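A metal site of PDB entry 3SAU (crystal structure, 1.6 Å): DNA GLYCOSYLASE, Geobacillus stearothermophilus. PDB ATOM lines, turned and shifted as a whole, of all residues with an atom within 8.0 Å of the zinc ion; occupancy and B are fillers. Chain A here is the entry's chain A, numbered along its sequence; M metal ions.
The zinc ion is bound by the side-chain sulfur of Cys 251 (2.3 Å), the side-chain sulfur of Cys 248 (2.3 Å) and the side-chain sulfur of Cys 268 (2.3 Å).
Slightly farther from the zinc ion lies SG of Cys 271 (3.0 Å).
SG of Cys 271 sits close to SG of Cys 251.
OG1 of Thr 253 lies close to SG of Cys 251 (3.3 Å).
SG of Cys 248 sits close to N of Arg 250 (3.4 Å).
The backbone NH (N) of Cys 248 sits at hydrogen-bond distance from the backbone carbonyl oxygen (O) of Thr 253.
SG of Cys 268 lies close to N of Cys 271.
N of Arg 270 sits close to SG of Cys 268 (3.5 Å).
The backbone NH (N) of Cys 268 sits at hydrogen-bond distance from the side-chain amide oxygen (OE1) of Gln 272 (2.8 Å).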
ATOM      1  N   PHE A 181      20.492 -13.079  21.319  1.00  0.00           N
ATOM      2  CA  PHE A 181      20.458 -11.783  20.626  1.00  0.00           C
ATOM      3  C   PHE A 181      21.465 -11.772  19.482  1.00  0.00           C
ATOM      4  O   PHE A 181      21.138 -11.349  18.368  1.00  0.00           O
ATOM      5  CB  PHE A 181      20.780 -10.635  21.585  1.00  0.00           C
ATOM      6  CG  PHE A 181      21.022  -9.341  20.877  1.00  0.00           C
ATOM      7  CD1 PHE A 181      19.965  -8.554  20.475  1.00  0.00           C
ATOM      8  CD2 PHE A 181      22.312  -8.935  20.573  1.00  0.00           C
ATOM      9  CE1 PHE A 181      20.176  -7.341  19.810  1.00  0.00           C
ATOM     10  CE2 PHE A 181      22.540  -7.734  19.898  1.00  0.00           C
ATOM     11  CZ  PHE A 181      21.474  -6.941  19.506  1.00  0.00           C
ATOM     12  N   TYR A 239      24.580  -6.543  25.320  1.00  0.00           N
ATOM     13  CA  TYR A 239      23.573  -6.079  24.364  1.00  0.00           C
ATOM     14  C   TYR A 239      22.172  -6.024  24.958  1.00  0.00           C
ATOM     15  O   TYR A 239      21.404  -5.098  24.661  1.00  0.00           O
ATOM     16  CB  TYR A 239      23.537  -6.992  23.136  1.00  0.00           C
ATOM     17  CG  TYR A 239      24.748  -6.876  22.262  1.00  0.00           C
ATOM     18  CD1 TYR A 239      25.765  -7.839  22.306  1.00  0.00           C
ATOM     19  CD2 TYR A 239      24.893  -5.805  21.374  1.00  0.00           C
ATOM     20  CE1 TYR A 239      26.880  -7.742  21.495  1.00  0.00           C
ATOM     21  CE2 TYR A 239      26.014  -5.701  20.565  1.00  0.00           C
ATOM     22  CZ  TYR A 239      26.998  -6.671  20.634  1.00  0.00           C
ATOM     23  OH  TYR A 239      28.105  -6.567  19.822  1.00  0.00           O
ATOM     24  N   VAL A 240      21.803  -7.034  25.746  1.00  0.00           N
ATOM     25  CA  VAL A 240      20.424  -7.109  26.227  1.00  0.00           C
ATOM     26  C   VAL A 240      20.282  -7.364  27.724  1.00  0.00           C
ATOM     27  O   VAL A 240      19.372  -6.844  28.350  1.00  0.00           O
ATOM     28  CB  VAL A 240      19.581  -8.154  25.445  1.00  0.00           C
ATOM     29  CG1 VAL A 240      19.507  -7.781  23.984  1.00  0.00           C
ATOM     30  CG2 VAL A 240      20.142  -9.569  25.620  1.00  0.00           C
ATOM     31  N   PRO A 247      17.871   1.583  24.828  1.00  0.00           N
ATOM     32  CA  PRO A 247      17.942   1.311  23.391  1.00  0.00           C
ATOM     33  C   PRO A 247      18.874   0.148  23.067  1.00  0.00           C
ATOM     34  O   PRO A 247      19.967   0.021  23.633  1.00  0.00           O
ATOM     35  CB  PRO A 247      18.536   2.604  22.806  1.00  0.00           C
ATOM     36  CG  PRO A 247      18.364   3.640  23.866  1.00  0.00           C
ATOM     37  CD  PRO A 247      18.417   2.917  25.168  1.00  0.00           C
ATOM     38  N   CYS A 248      18.433  -0.693  22.142  1.00  0.00           N
ATOM     39  CA  CYS A 248      19.284  -1.725  21.580  1.00  0.00           C
ATOM     40  C   CYS A 248      20.503  -1.041  20.982  1.00  0.00           C
ATOM     41  O   CYS A 248      20.404  -0.004  20.336  1.00  0.00           O
ATOM     42  CB  CYS A 248      18.513  -2.477  20.500  1.00  0.00           C
ATOM     43  SG  CYS A 248      19.466  -3.736  19.617  1.00  0.00           S
ATOM     44  N   LYS A 249      21.672  -1.639  21.211  1.00  0.00           N
ATOM     45  CA  LYS A 249      22.923  -1.053  20.746  1.00  0.00           C
ATOM     46  C   LYS A 249      23.102  -1.262  19.246  1.00  0.00           C
ATOM     47  O   LYS A 249      23.975  -0.643  18.630  1.00  0.00           O
ATOM     48  CB  LYS A 249      24.106  -1.669  21.499  1.00  0.00           C
ATOM     49  CG  LYS A 249      24.082  -1.357  22.982  1.00  0.00           C
ATOM     50  CD  LYS A 249      25.306  -1.928  23.698  1.00  0.00           C
ATOM     51  CE  LYS A 249      25.358  -1.435  25.133  1.00  0.00           C
ATOM     52  NZ  LYS A 249      26.574  -1.907  25.855  1.00  0.00           N
ATOM     53  N   ARG A 250      22.253  -2.109  18.662  1.00  0.00           N
ATOM     54  CA  ARG A 250      22.322  -2.383  17.235  1.00  0.00           C
ATOM     55  C   ARG A 250      21.264  -1.606  16.450  1.00  0.00           C
ATOM     56  O   ARG A 250      21.530  -1.184  15.324  1.00  0.00           O
ATOM     57  CB  ARG A 250      22.172  -3.898  17.003  1.00  0.00           C
ATOM     58  CG  ARG A 250      22.290  -4.345  15.564  1.00  0.00           C
ATOM     59  CD  ARG A 250      22.838  -5.779  15.537  1.00  0.00           C
ATOM     60  NE  ARG A 250      24.119  -5.853  16.238  1.00  0.00           N
ATOM     61  CZ  ARG A 250      24.739  -6.982  16.587  1.00  0.00           C
ATOM     62  NH1 ARG A 250      24.194  -8.159  16.306  1.00  0.00           N
ATOM     63  NH2 ARG A 250      25.904  -6.931  17.208  1.00  0.00           N
ATOM     64  N   CYS A 251      20.063  -1.441  17.015  1.00  0.00           N
ATOM     65  CA  CYS A 251      18.984  -0.811  16.242  1.00  0.00           C
ATOM     66  C   CYS A 251      18.226   0.316  16.930  1.00  0.00           C
ATOM     67  O   CYS A 251      17.390   0.987  16.308  1.00  0.00           O
ATOM     68  CB  CYS A 251      17.962  -1.858  15.768  1.00  0.00           C
ATOM     69  SG  CYS A 251      16.886  -2.468  17.103  1.00  0.00           S
ATOM     70  N   GLY A 252      18.488   0.513  18.225  1.00  0.00           N
ATOM     71  CA  GLY A 252      17.852   1.584  18.975  1.00  0.00           C
ATOM     72  C   GLY A 252      16.488   1.269  19.571  1.00  0.00           C
ATOM     73  O   GLY A 252      15.949   2.055  20.360  1.00  0.00           O
ATOM     74  N   THR A 253      15.904   0.135  19.177  1.00  0.00           N
ATOM     75  CA  THR A 253      14.620  -0.304  19.735  1.00  0.00           C
ATOM     76  C   THR A 253      14.814  -0.613  21.227  1.00  0.00           C
ATOM     77  O   THR A 253      15.792  -1.247  21.612  1.00  0.00           O
ATOM     78  CB  THR A 253      14.120  -1.563  19.003  1.00  0.00           C
ATOM     79  OG1 THR A 253      13.893  -1.259  17.618  1.00  0.00           O
ATOM     80  CG2 THR A 253      12.809  -2.077  19.615  1.00  0.00           C
ATOM     81  N   PRO A 254      13.888  -0.168  22.084  1.00  0.00           N
ATOM     82  CA  PRO A 254      14.061  -0.502  23.497  1.00  0.00           C
ATOM     83  C   PRO A 254      14.086  -2.003  23.760  1.00  0.00           C
ATOM     84  O   PRO A 254      13.240  -2.753  23.246  1.00  0.00           O
ATOM     85  CB  PRO A 254      12.827   0.117  24.168  1.00  0.00           C
ATOM     86  CG  PRO A 254      12.449   1.237  23.251  1.00  0.00           C
ATOM     87  CD  PRO A 254      12.741   0.733  21.862  1.00  0.00           C
ATOM     88  N   ILE A 255      15.038  -2.427  24.569  1.00  0.00           N
ATOM     89  CA  ILE A 255      15.118  -3.814  24.965  1.00  0.00           C
ATOM     90  C   ILE A 255      13.944  -4.163  25.876  1.00  0.00           C
ATOM     91  O   ILE A 255      13.513  -3.357  26.697  1.00  0.00           O
ATOM     92  CB  ILE A 255      16.457  -4.082  25.652  1.00  0.00           C
ATOM     93  CG1 ILE A 255      17.601  -3.816  24.659  1.00  0.00           C
ATOM     94  CG2 ILE A 255      16.505  -5.501  26.232  1.00  0.00           C
ATOM     95  CD1 ILE A 255      17.447  -4.592  23.321  1.00  0.00           C
ATOM     96  N   TYR A 267      15.505  -9.260  25.508  1.00  0.00           N
ATOM     97  CA  TYR A 267      15.656  -9.438  24.071  1.00  0.00           C
ATOM     98  C   TYR A 267      15.315  -8.148  23.324  1.00  0.00           C
ATOM     99  O   TYR A 267      14.637  -7.253  23.851  1.00  0.00           O
ATOM    100  CB  TYR A 267      14.769 -10.590  23.570  1.00  0.00           C
ATOM    101  CG  TYR A 267      13.285 -10.347  23.802  1.00  0.00           C
ATOM    102  CD1 TYR A 267      12.487  -9.826  22.790  1.00  0.00           C
ATOM    103  CD2 TYR A 267      12.696 -10.622  25.033  1.00  0.00           C
ATOM    104  CE1 TYR A 267      11.141  -9.593  22.981  1.00  0.00           C
ATOM    105  CE2 TYR A 267      11.333 -10.378  25.234  1.00  0.00           C
ATOM    106  CZ  TYR A 267      10.567  -9.865  24.205  1.00  0.00           C
ATOM    107  OH  TYR A 267       9.223  -9.615  24.379  1.00  0.00           O
ATOM    108  N   CYS A 268      15.780  -8.049  22.083  1.00  0.00           N
ATOM    109  CA  CYS A 268      15.350  -6.973  21.190  1.00  0.00           C
ATOM    110  C   CYS A 268      14.262  -7.524  20.278  1.00  0.00           C
ATOM    111  O   CYS A 268      14.485  -8.508  19.555  1.00  0.00           O
ATOM    112  CB  CYS A 268      16.516  -6.479  20.355  1.00  0.00           C
ATOM    113  SG  CYS A 268      15.982  -5.317  19.090  1.00  0.00           S
ATOM    114  N   PRO A 269      13.068  -6.932  20.343  1.00  0.00           N
ATOM    115  CA  PRO A 269      11.920  -7.472  19.598  1.00  0.00           C
ATOM    116  C   PRO A 269      12.017  -7.192  18.099  1.00  0.00           C
ATOM    117  O   PRO A 269      11.285  -7.801  17.309  1.00  0.00           O
ATOM    118  CB  PRO A 269      10.736  -6.733  20.226  1.00  0.00           C
ATOM    119  CG  PRO A 269      11.330  -5.447  20.710  1.00  0.00           C
ATOM    120  CD  PRO A 269      12.656  -5.871  21.285  1.00  0.00           C
ATOM    121  N   ARG A 270      12.912  -6.297  17.700  1.00  0.00           N
ATOM    122  CA  ARG A 270      13.105  -6.028  16.277  1.00  0.00           C
ATOM    123  C   ARG A 270      14.088  -7.000  15.645  1.00  0.00           C
ATOM    124  O   ARG A 270      13.845  -7.522  14.553  1.00  0.00           O
ATOM    125  CB  ARG A 270      13.618  -4.606  16.050  1.00  0.00           C
ATOM    126  CG  ARG A 270      13.889  -4.340  14.558  1.00  0.00           C
ATOM    127  CD  ARG A 270      14.361  -2.921  14.282  1.00  0.00           C
ATOM    128  NE  ARG A 270      14.680  -2.765  12.872  1.00  0.00           N
ATOM    129  CZ  ARG A 270      14.905  -1.611  12.270  1.00  0.00           C
ATOM    130  NH1 ARG A 270      15.162  -1.586  10.969  1.00  0.00           N
ATOM    131  NH2 ARG A 270      14.872  -0.467  12.962  1.00  0.00           N
ATOM    132  N   CYS A 271      15.197  -7.259  16.324  1.00  0.00           N
ATOM    133  CA  CYS A 271      16.282  -8.005  15.729  1.00  0.00           C
ATOM    134  C   CYS A 271      16.297  -9.501  16.002  1.00  0.00           C
ATOM    135  O   CYS A 271      17.017 -10.228  15.348  1.00  0.00           O
ATOM    136  CB  CYS A 271      17.590  -7.410  16.131  1.00  0.00           C
ATOM    137  SG  CYS A 271      17.609  -5.712  15.518  1.00  0.00           S
ATOM    138  N   GLN A 272      15.513  -9.932  16.976  1.00  0.00           N
ATOM    139  CA  GLN A 272      15.382 -11.352  17.237  1.00  0.00           C
ATOM    140  C   GLN A 272      14.037 -11.824  16.717  1.00  0.00           C
ATOM    141  O   GLN A 272      13.017 -11.135  16.901  1.00  0.00           O
ATOM    142  CB  GLN A 272      15.537 -11.645  18.736  1.00  0.00           C
ATOM    143  CG  GLN A 272      16.953 -11.413  19.226  1.00  0.00           C
ATOM    144  CD  GLN A 272      17.080 -11.416  20.740  1.00  0.00           C
ATOM    145  OE1 GLN A 272      17.219 -10.366  21.352  1.00  0.00           O
ATOM    146  NE2 GLN A 272      17.056 -12.611  21.359  1.00  0.00           N
HETATM  147 ZN    ZN M   1      17.834  -4.304  18.103  1.00  0.00          ZN
